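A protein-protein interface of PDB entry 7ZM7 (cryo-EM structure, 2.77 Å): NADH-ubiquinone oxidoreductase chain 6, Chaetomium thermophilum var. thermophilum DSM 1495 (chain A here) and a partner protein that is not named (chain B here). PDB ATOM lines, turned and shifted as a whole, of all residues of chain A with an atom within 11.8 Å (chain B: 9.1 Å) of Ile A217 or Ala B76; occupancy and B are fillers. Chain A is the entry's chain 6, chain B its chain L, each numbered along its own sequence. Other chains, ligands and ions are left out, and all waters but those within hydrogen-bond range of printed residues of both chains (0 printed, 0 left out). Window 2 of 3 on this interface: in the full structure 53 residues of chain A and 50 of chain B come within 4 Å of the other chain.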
ATOM      1  N   LEU A  84     -15.537   5.042  34.562  1.00  0.00           N
ATOM      2  CA  LEU A  84     -15.530   5.948  33.424  1.00  0.00           C
ATOM      3  C   LEU A  84     -14.657   7.165  33.704  1.00  0.00           C
ATOM      4  O   LEU A  84     -13.960   7.657  32.813  1.00  0.00           O
ATOM      5  CB  LEU A  84     -16.959   6.355  33.085  1.00  0.00           C
ATOM      6  CG  LEU A  84     -17.237   6.919  31.691  1.00  0.00           C
ATOM      7  CD1 LEU A  84     -16.486   6.139  30.643  1.00  0.00           C
ATOM      8  CD2 LEU A  84     -18.713   6.928  31.403  1.00  0.00           C
ATOM      9  N   ILE A  88     -11.145   8.163  31.409  1.00  0.00           N
ATOM     10  CA  ILE A  88     -10.848   9.459  30.820  1.00  0.00           C
ATOM     11  C   ILE A  88      -9.614  10.074  31.468  1.00  0.00           C
ATOM     12  O   ILE A  88      -8.766  10.653  30.788  1.00  0.00           O
ATOM     13  CB  ILE A  88     -12.073  10.384  30.912  1.00  0.00           C
ATOM     14  CG1 ILE A  88     -13.238   9.760  30.164  1.00  0.00           C
ATOM     15  CG2 ILE A  88     -11.761  11.746  30.345  1.00  0.00           C
ATOM     16  CD1 ILE A  88     -12.948   9.530  28.717  1.00  0.00           C
ATOM     17  N   ILE A  92      -6.521  11.254  28.914  1.00  0.00           N
ATOM     18  CA  ILE A  92      -6.242  12.666  28.729  1.00  0.00           C
ATOM     19  C   ILE A  92      -4.852  12.975  29.255  1.00  0.00           C
ATOM     20  O   ILE A  92      -4.440  12.487  30.315  1.00  0.00           O
ATOM     21  CB  ILE A  92      -7.312  13.512  29.433  1.00  0.00           C
ATOM     22  CG1 ILE A  92      -8.611  13.480  28.636  1.00  0.00           C
ATOM     23  CG2 ILE A  92      -6.828  14.910  29.657  1.00  0.00           C
ATOM     24  CD1 ILE A  92      -9.649  14.440  29.151  1.00  0.00           C
ATOM     25  N   LEU A 208     -32.097   7.148  27.857  1.00  0.00           N
ATOM     26  CA  LEU A 208     -32.106   7.016  26.408  1.00  0.00           C
ATOM     27  C   LEU A 208     -31.505   8.242  25.725  1.00  0.00           C
ATOM     28  O   LEU A 208     -30.866   8.124  24.678  1.00  0.00           O
ATOM     29  CB  LEU A 208     -33.540   6.778  25.939  1.00  0.00           C
ATOM     30  CG  LEU A 208     -33.846   6.756  24.454  1.00  0.00           C
ATOM     31  CD1 LEU A 208     -33.208   5.559  23.841  1.00  0.00           C
ATOM     32  CD2 LEU A 208     -35.313   6.697  24.254  1.00  0.00           C
ATOM     33  N   LEU A 209     -31.724   9.430  26.287  1.00  0.00           N
ATOM     34  CA  LEU A 209     -31.106  10.634  25.748  1.00  0.00           C
ATOM     35  C   LEU A 209     -29.602  10.652  26.008  1.00  0.00           C
ATOM     36  O   LEU A 209     -28.826  11.082  25.151  1.00  0.00           O
ATOM     37  CB  LEU A 209     -31.780  11.872  26.336  1.00  0.00           C
ATOM     38  CG  LEU A 209     -31.075  13.219  26.147  1.00  0.00           C
ATOM     39  CD1 LEU A 209     -31.231  13.705  24.735  1.00  0.00           C
ATOM     40  CD2 LEU A 209     -31.579  14.258  27.135  1.00  0.00           C
ATOM     41  N   ALA A 210     -29.172  10.195  27.177  1.00  0.00           N
ATOM     42  CA  ALA A 210     -27.752  10.115  27.468  1.00  0.00           C
ATOM     43  C   ALA A 210     -27.044   9.067  26.623  1.00  0.00           C
ATOM     44  O   ALA A 210     -25.820   9.103  26.516  1.00  0.00           O
ATOM     45  CB  ALA A 210     -27.547   9.839  28.955  1.00  0.00           C
ATOM     46  N   MET A 211     -27.782   8.128  26.036  1.00  0.00           N
ATOM     47  CA  MET A 211     -27.193   7.203  25.078  1.00  0.00           C
ATOM     48  C   MET A 211     -26.998   7.872  23.730  1.00  0.00           C
ATOM     49  O   MET A 211     -25.881   7.957  23.218  1.00  0.00           O
ATOM     50  CB  MET A 211     -28.076   5.968  24.931  1.00  0.00           C
ATOM     51  CG  MET A 211     -27.600   4.987  23.881  1.00  0.00           C
ATOM     52  SD  MET A 211     -26.312   3.894  24.502  1.00  0.00           S
ATOM     53  CE  MET A 211     -27.307   2.628  25.280  1.00  0.00           C
ATOM     54  N   VAL A 212     -28.083   8.373  23.154  1.00  0.00           N
ATOM     55  CA  VAL A 212     -28.042   8.944  21.815  1.00  0.00           C
ATOM     56  C   VAL A 212     -27.140  10.166  21.780  1.00  0.00           C
ATOM     57  O   VAL A 212     -26.333  10.331  20.862  1.00  0.00           O
ATOM     58  CB  VAL A 212     -29.468   9.281  21.358  1.00  0.00           C
ATOM     59  CG1 VAL A 212     -29.460  10.160  20.128  1.00  0.00           C
ATOM     60  CG2 VAL A 212     -30.238   8.007  21.125  1.00  0.00           C
ATOM     61  N   GLY A 213     -27.270  11.043  22.773  1.00  0.00           N
ATOM     62  CA  GLY A 213     -26.534  12.289  22.743  1.00  0.00           C
ATOM     63  C   GLY A 213     -25.041  12.110  22.909  1.00  0.00           C
ATOM     64  O   GLY A 213     -24.250  12.804  22.273  1.00  0.00           O
ATOM     65  N   ALA A 214     -24.630  11.220  23.797  1.00  0.00           N
ATOM     66  CA  ALA A 214     -23.204  11.061  24.035  1.00  0.00           C
ATOM     67  C   ALA A 214     -22.530  10.284  22.917  1.00  0.00           C
ATOM     68  O   ALA A 214     -21.357  10.523  22.619  1.00  0.00           O
ATOM     69  CB  ALA A 214     -22.980  10.390  25.383  1.00  0.00           C
ATOM     70  N   ILE A 215     -23.253   9.367  22.281  1.00  0.00           N
ATOM     71  CA  ILE A 215     -22.726   8.696  21.102  1.00  0.00           C
ATOM     72  C   ILE A 215     -22.593   9.678  19.943  1.00  0.00           C
ATOM     73  O   ILE A 215     -21.591   9.667  19.224  1.00  0.00           O
ATOM     74  CB  ILE A 215     -23.606   7.481  20.750  1.00  0.00           C
ATOM     75  CG1 ILE A 215     -23.319   6.334  21.722  1.00  0.00           C
ATOM     76  CG2 ILE A 215     -23.365   7.021  19.324  1.00  0.00           C
ATOM     77  CD1 ILE A 215     -24.315   5.192  21.666  1.00  0.00           C
ATOM     78  N   VAL A 216     -23.573  10.567  19.759  1.00  0.00           N
ATOM     79  CA  VAL A 216     -23.565  11.439  18.590  1.00  0.00           C
ATOM     80  C   VAL A 216     -22.530  12.553  18.697  1.00  0.00           C
ATOM     81  O   VAL A 216     -22.126  13.112  17.677  1.00  0.00           O
ATOM     82  CB  VAL A 216     -24.963  12.037  18.324  1.00  0.00           C
ATOM     83  CG1 VAL A 216     -25.348  13.021  19.388  1.00  0.00           C
ATOM     84  CG2 VAL A 216     -25.030  12.688  16.965  1.00  0.00           C
ATOM     85  N   ILE A 217     -22.070  12.907  19.896  1.00  0.00           N
ATOM     86  CA  ILE A 217     -21.098  13.986  20.006  1.00  0.00           C
ATOM     87  C   ILE A 217     -19.674  13.484  20.111  1.00  0.00           C
ATOM     88  O   ILE A 217     -18.753  14.295  20.192  1.00  0.00           O
ATOM     89  CB  ILE A 217     -21.409  14.931  21.183  1.00  0.00           C
ATOM     90  CG1 ILE A 217     -21.264  14.206  22.515  1.00  0.00           C
ATOM     91  CG2 ILE A 217     -22.773  15.570  21.003  1.00  0.00           C
ATOM     92  CD1 ILE A 217     -21.096  15.107  23.696  1.00  0.00           C
ATOM     93  N   THR A 218     -19.456  12.180  20.084  1.00  0.00           N
ATOM     94  CA  THR A 218     -18.099  11.667  20.200  1.00  0.00           C
ATOM     95  C   THR A 218     -17.639  10.895  18.974  1.00  0.00           C
ATOM     96  O   THR A 218     -16.508  11.093  18.529  1.00  0.00           O
ATOM     97  CB  THR A 218     -17.941  10.798  21.469  1.00  0.00           C
ATOM     98  OG1 THR A 218     -19.035   9.884  21.585  1.00  0.00           O
ATOM     99  CG2 THR A 218     -17.853  11.662  22.709  1.00  0.00           C
ATOM    100  N   ILE A 219     -18.449  10.030  18.413  1.00  0.00           N
ATOM    101  CA  ILE A 219     -17.920   9.118  17.420  1.00  0.00           C
ATOM    102  C   ILE A 219     -17.975   9.782  16.054  1.00  0.00           C
ATOM    103  O   ILE A 219     -18.805  10.642  15.781  1.00  0.00           O
ATOM    104  CB  ILE A 219     -18.648   7.762  17.380  1.00  0.00           C
ATOM    105  CG1 ILE A 219     -20.105   7.916  16.987  1.00  0.00           C
ATOM    106  CG2 ILE A 219     -18.601   7.098  18.739  1.00  0.00           C
ATOM    107  CD1 ILE A 219     -20.757   6.588  16.714  1.00  0.00           C
ATOM    108  N   LYS A 220     -17.049   9.387  15.201  1.00  0.00           N
ATOM    109  CA  LYS A 220     -17.123   9.689  13.790  1.00  0.00           C
ATOM    110  C   LYS A 220     -18.045   8.670  13.140  1.00  0.00           C
ATOM    111  O   LYS A 220     -17.793   7.470  13.259  1.00  0.00           O
ATOM    112  CB  LYS A 220     -15.739   9.627  13.170  1.00  0.00           C
ATOM    113  CG  LYS A 220     -15.673   9.826  11.681  1.00  0.00           C
ATOM    114  CD  LYS A 220     -15.919  11.257  11.291  1.00  0.00           C
ATOM    115  CE  LYS A 220     -15.944  11.402   9.783  1.00  0.00           C
ATOM    116  NZ  LYS A 220     -14.614  11.097   9.184  1.00  0.00           N
ATOM    117  N   PRO A 221     -19.127   9.085  12.488  1.00  0.00           N
ATOM    118  CA  PRO A 221     -20.038   8.104  11.891  1.00  0.00           C
ATOM    119  C   PRO A 221     -19.343   7.273  10.826  1.00  0.00           C
ATOM    120  O   PRO A 221     -18.491   7.763  10.082  1.00  0.00           O
ATOM    121  CB  PRO A 221     -21.151   8.970  11.285  1.00  0.00           C
ATOM    122  CG  PRO A 221     -21.028  10.278  11.953  1.00  0.00           C
ATOM    123  CD  PRO A 221     -19.584  10.463  12.263  1.00  0.00           C
ATOM    124  N   ARG A 222     -19.721   6.000  10.763  1.00  0.00           N
ATOM    125  CA  ARG A 222     -19.147   5.052   9.811  1.00  0.00           C
ATOM    126  C   ARG A 222     -17.635   4.946   9.972  1.00  0.00           C
ATOM    127  O   ARG A 222     -16.992   4.114   9.333  1.00  0.00           O
ATOM    128  CB  ARG A 222     -19.493   5.447   8.372  1.00  0.00           C
ATOM    129  N   ALA B  68     -22.135  10.698  32.150  1.00  0.00           N
ATOM    130  CA  ALA B  68     -21.959  10.295  30.739  1.00  0.00           C
ATOM    131  C   ALA B  68     -21.975  11.515  29.835  1.00  0.00           C
ATOM    132  O   ALA B  68     -21.088  11.622  28.977  1.00  0.00           O
ATOM    133  CB  ALA B  68     -23.089   9.390  30.320  1.00  0.00           C
ATOM    134  N   ILE B  69     -22.949  12.395  30.034  1.00  0.00           N
ATOM    135  CA  ILE B  69     -23.067  13.617  29.190  1.00  0.00           C
ATOM    136  C   ILE B  69     -21.863  14.515  29.484  1.00  0.00           C
ATOM    137  O   ILE B  69     -21.313  15.065  28.540  1.00  0.00           O
ATOM    138  CB  ILE B  69     -24.444  14.276  29.432  1.00  0.00           C
ATOM    139  CG1 ILE B  69     -25.589  13.358  29.006  1.00  0.00           C
ATOM    140  CG2 ILE B  69     -24.537  15.631  28.748  1.00  0.00           C
ATOM    141  CD1 ILE B  69     -25.529  12.959  27.558  1.00  0.00           C
ATOM    142  N   GLY B  70     -21.477  14.637  30.754  1.00  0.00           N
ATOM    143  CA  GLY B  70     -20.352  15.485  31.177  1.00  0.00           C
ATOM    144  C   GLY B  70     -18.996  15.020  30.701  1.00  0.00           C
ATOM    145  O   GLY B  70     -18.164  15.870  30.365  1.00  0.00           O
ATOM    146  N   LEU B  71     -18.762  13.706  30.749  1.00  0.00           N
ATOM    147  CA  LEU B  71     -17.472  13.163  30.285  1.00  0.00           C
ATOM    148  C   LEU B  71     -17.519  13.062  28.761  1.00  0.00           C
ATOM    149  O   LEU B  71     -16.459  13.197  28.146  1.00  0.00           O
ATOM    150  CB  LEU B  71     -17.187  11.842  30.993  1.00  0.00           C
ATOM    151  CG  LEU B  71     -16.740  11.973  32.448  1.00  0.00           C
ATOM    152  CD1 LEU B  71     -16.635  10.611  33.112  1.00  0.00           C
ATOM    153  CD2 LEU B  71     -15.422  12.722  32.543  1.00  0.00           C
ATOM    154  N   GLY B  72     -18.704  12.888  28.178  1.00  0.00           N
ATOM    155  CA  GLY B  72     -18.773  12.920  26.730  1.00  0.00           C
ATOM    156  C   GLY B  72     -18.465  14.283  26.149  1.00  0.00           C
ATOM    157  O   GLY B  72     -17.766  14.390  25.137  1.00  0.00           O
ATOM    158  N   ILE B  73     -19.012  15.338  26.751  1.00  0.00           N
ATOM    159  CA  ILE B  73     -18.752  16.689  26.277  1.00  0.00           C
ATOM    160  C   ILE B  73     -17.306  17.067  26.541  1.00  0.00           C
ATOM    161  O   ILE B  73     -16.669  17.755  25.737  1.00  0.00           O
ATOM    162  CB  ILE B  73     -19.740  17.677  26.930  1.00  0.00           C
ATOM    163  CG1 ILE B  73     -21.121  17.528  26.308  1.00  0.00           C
ATOM    164  CG2 ILE B  73     -19.293  19.121  26.782  1.00  0.00           C
ATOM    165  CD1 ILE B  73     -22.188  18.276  27.030  1.00  0.00           C
ATOM    166  N   LEU B  74     -16.764  16.637  27.676  1.00  0.00           N
ATOM    167  CA  LEU B  74     -15.365  16.901  27.965  1.00  0.00           C
ATOM    168  C   LEU B  74     -14.439  16.184  26.988  1.00  0.00           C
ATOM    169  O   LEU B  74     -13.315  16.633  26.759  1.00  0.00           O
ATOM    170  CB  LEU B  74     -15.044  16.497  29.394  1.00  0.00           C
ATOM    171  CG  LEU B  74     -13.626  16.789  29.842  1.00  0.00           C
ATOM    172  CD1 LEU B  74     -13.524  18.188  30.389  1.00  0.00           C
ATOM    173  CD2 LEU B  74     -13.167  15.753  30.837  1.00  0.00           C
ATOM    174  N   VAL B  75     -14.868  15.051  26.439  1.00  0.00           N
ATOM    175  CA  VAL B  75     -14.079  14.393  25.408  1.00  0.00           C
ATOM    176  C   VAL B  75     -14.112  15.200  24.124  1.00  0.00           C
ATOM    177  O   VAL B  75     -13.077  15.447  23.503  1.00  0.00           O
ATOM    178  CB  VAL B  75     -14.575  12.955  25.170  1.00  0.00           C
ATOM    179  CG1 VAL B  75     -14.106  12.471  23.828  1.00  0.00           C
ATOM    180  CG2 VAL B  75     -14.087  12.044  26.244  1.00  0.00           C
ATOM    181  N   ALA B  76     -15.299  15.660  23.734  1.00  0.00           N
ATOM    182  CA  ALA B  76     -15.456  16.468  22.503  1.00  0.00           C
ATOM    183  C   ALA B  76     -14.578  17.720  22.583  1.00  0.00           C
ATOM    184  O   ALA B  76     -13.958  18.082  21.564  1.00  0.00           O
ATOM    185  CB  ALA B  76     -16.908  16.813  22.337  1.00  0.00           C
ATOM    186  N   PHE B  77     -14.519  18.354  23.752  1.00  0.00           N
ATOM    187  CA  PHE B  77     -13.684  19.558  23.972  1.00  0.00           C
ATOM    188  C   PHE B  77     -12.203  19.194  23.848  1.00  0.00           C
ATOM    189  O   PHE B  77     -11.496  19.878  23.096  1.00  0.00           O
ATOM    190  CB  PHE B  77     -14.073  20.175  25.319  1.00  0.00           C
ATOM    191  CG  PHE B  77     -13.260  21.361  25.767  1.00  0.00           C
ATOM    192  CD1 PHE B  77     -13.502  22.623  25.252  1.00  0.00           C
ATOM    193  CD2 PHE B  77     -12.271  21.217  26.725  1.00  0.00           C
ATOM    194  CE1 PHE B  77     -12.759  23.712  25.672  1.00  0.00           C
ATOM    195  CE2 PHE B  77     -11.531  22.308  27.147  1.00  0.00           C
ATOM    196  CZ  PHE B  77     -11.777  23.552  26.619  1.00  0.00           C
ATOM    197  N   TYR B  78     -11.752  18.147  24.539  1.00  0.00           N
ATOM    198  CA  TYR B  78     -10.323  17.731  24.538  1.00  0.00           C
ATOM    199  C   TYR B  78      -9.830  17.388  23.126  1.00  0.00           C
ATOM    200  O   TYR B  78      -8.671  17.684  22.843  1.00  0.00           O
ATOM    201  CB  TYR B  78     -10.131  16.583  25.532  1.00  0.00           C
ATOM    202  CG  TYR B  78      -8.762  15.955  25.546  1.00  0.00           C
ATOM    203  CD1 TYR B  78      -7.698  16.560  26.193  1.00  0.00           C
ATOM    204  CD2 TYR B  78      -8.540  14.742  24.922  1.00  0.00           C
ATOM    205  CE1 TYR B  78      -6.440  15.984  26.200  1.00  0.00           C
ATOM    206  CE2 TYR B  78      -7.290  14.151  24.921  1.00  0.00           C
ATOM    207  CZ  TYR B  78      -6.237  14.773  25.564  1.00  0.00           C
ATOM    208  OH  TYR B  78      -5.011  14.178  25.562  1.00  0.00           O
ATOM    209  N   ARG B  79     -10.668  16.796  22.277  1.00  0.00           N
ATOM    210  CA  ARG B  79     -10.253  16.366  20.920  1.00  0.00           C
ATOM    211  C   ARG B  79      -9.732  17.576  20.136  1.00  0.00           C
ATOM    212  O   ARG B  79      -8.732  17.424  19.416  1.00  0.00           O
ATOM    213  CB  ARG B  79     -11.451  15.762  20.179  1.00  0.00           C
ATOM    214  CG  ARG B  79     -11.113  15.153  18.828  1.00  0.00           C
ATOM    215  CD  ARG B  79     -12.222  14.275  18.293  1.00  0.00           C
ATOM    216  NE  ARG B  79     -13.279  15.109  17.762  1.00  0.00           N
ATOM    217  CZ  ARG B  79     -13.448  15.380  16.476  1.00  0.00           C
ATOM    218  NH1 ARG B  79     -14.438  16.165  16.101  1.00  0.00           N
ATOM    219  NH2 ARG B  79     -12.652  14.849  15.570  1.00  0.00           N
ATOM    220  N   LEU B  80     -10.392  18.732  20.267  1.00  0.00           N
ATOM    221  CA  LEU B  80      -9.967  19.948  19.536  1.00  0.00           C
ATOM    222  C   LEU B  80      -9.021  20.821  20.365  1.00  0.00           C
ATOM    223  O   LEU B  80      -8.381  21.692  19.774  1.00  0.00           O
ATOM    224  CB  LEU B  80     -11.216  20.720  19.105  1.00  0.00           C
ATOM    225  CG  LEU B  80     -12.342  19.865  18.530  1.00  0.00           C
ATOM    226  CD1 LEU B  80     -13.597  20.694  18.321  1.00  0.00           C
ATOM    227  CD2 LEU B  80     -11.917  19.206  17.230  1.00  0.00           C
ATOM    228  N   ARG B  81      -8.955  20.557  21.705  1.00  0.00           N
ATOM    229  CA  ARG B  81      -8.139  21.464  22.552  1.00  0.00           C
ATOM    230  C   ARG B  81      -6.778  20.819  22.840  1.00  0.00           C
ATOM    231  O   ARG B  81      -5.759  21.482  22.598  1.00  0.00           O
ATOM    232  CB  ARG B  81      -8.923  21.884  23.800  1.00  0.00           C
ATOM    233  CG  ARG B  81      -8.318  23.041  24.578  1.00  0.00           C
ATOM    234  CD  ARG B  81      -8.881  24.382  24.163  1.00  0.00           C
ATOM    235  NE  ARG B  81      -8.759  25.355  25.237  1.00  0.00           N
ATOM    236  CZ  ARG B  81      -9.058  26.643  25.124  1.00  0.00           C
ATOM    237  NH1 ARG B  81      -9.485  27.125  23.970  1.00  0.00           N
ATOM    238  NH2 ARG B  81      -8.914  27.447  26.162  1.00  0.00           N
ATOM    239  N   GLY B  82      -6.736  19.590  23.271  1.00  0.00           N
ATOM    240  CA  GLY B  82      -5.482  18.919  23.668  1.00  0.00           C
ATOM    241  C   GLY B  82      -5.095  19.242  25.085  1.00  0.00           C
ATOM    242  O   GLY B  82      -3.989  18.875  25.481  1.00  0.00           O
ATOM    243  N   SER B  83      -5.989  19.895  25.819  1.00  0.00           N
ATOM    244  CA  SER B  83      -5.700  20.311  27.208  1.00  0.00           C
ATOM    245  C   SER B  83      -7.017  20.590  27.927  1.00  0.00           C
ATOM    246  O   SER B  83      -7.921  21.149  27.295  1.00  0.00           O
ATOM    247  CB  SER B  83      -4.811  21.509  27.227  1.00  0.00           C
ATOM    248  OG  SER B  83      -4.349  21.769  28.541  1.00  0.00           O
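O of Leu A84 touches CD1 of Leu B71, at 3.996 Å.
CD1 of Ile A88 touches CG2 of Val B75, 3.7 Å away.
CG2 of Ile A92 touches CE1 of Tyr B78, 3.6 Å away.
Ala A210 touches Ile B69.
Ile A217 touches Gly B72.
Ile A217 touches Ile B73.
Ala B76 touches Ile A217.
CG2 of Thr A218 touches O of Gly B72, at 3.7 Å.
Thr A218 touches Val B75.
O of Ala A214 sits at hydrogen-bond distance from OG1 of Thr A218, 2.6 Å away.
O of Ile A215 sits at hydrogen-bond distance from OG1 of Thr A218 (3.5 Å).
Ile A217 touches just these residues of chain B: Gly B72, Ile B73 and Ala B76.
Ala B76 touches one residue of chain A.
No residue of chain B comes within 4 Å of Val A216.
No residue of chain A comes within 4 Å of Gly B70.
Of chain A, only Ile A217 (3.7 Å) and Thr A218 (3.7 Å) come within 4 Å of Gly B72.
Leu B74 touches none of the printed residues of chain A.
Of the printed residues of chain B, Ile A92 touches Tyr B78 (3.6 Å).
Of the printed residues of chain A, Leu B71 touches Leu A84.
Of the printed residues of chain B, Leu A84 touches Leu B71.
Of the printed residues of chain A, Tyr B78 touches Ile A92 (3.6 Å).
Printed residues of chain B within 4 Å of Ile A88: Val B75 (3.7 Å).
The nearest residue of chain A that does not touch Ala B76 is Thr A218 (4.9 Å).
The nearest printed residue of chain B that does not touch Ile A92 is Leu B74 (4.1 Å).
Hydrophobic or aromatic side chains of chain A within 4 Å of the printed part of chain B: Ile A88, Ile A92, Ala A210 and Ile A217.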
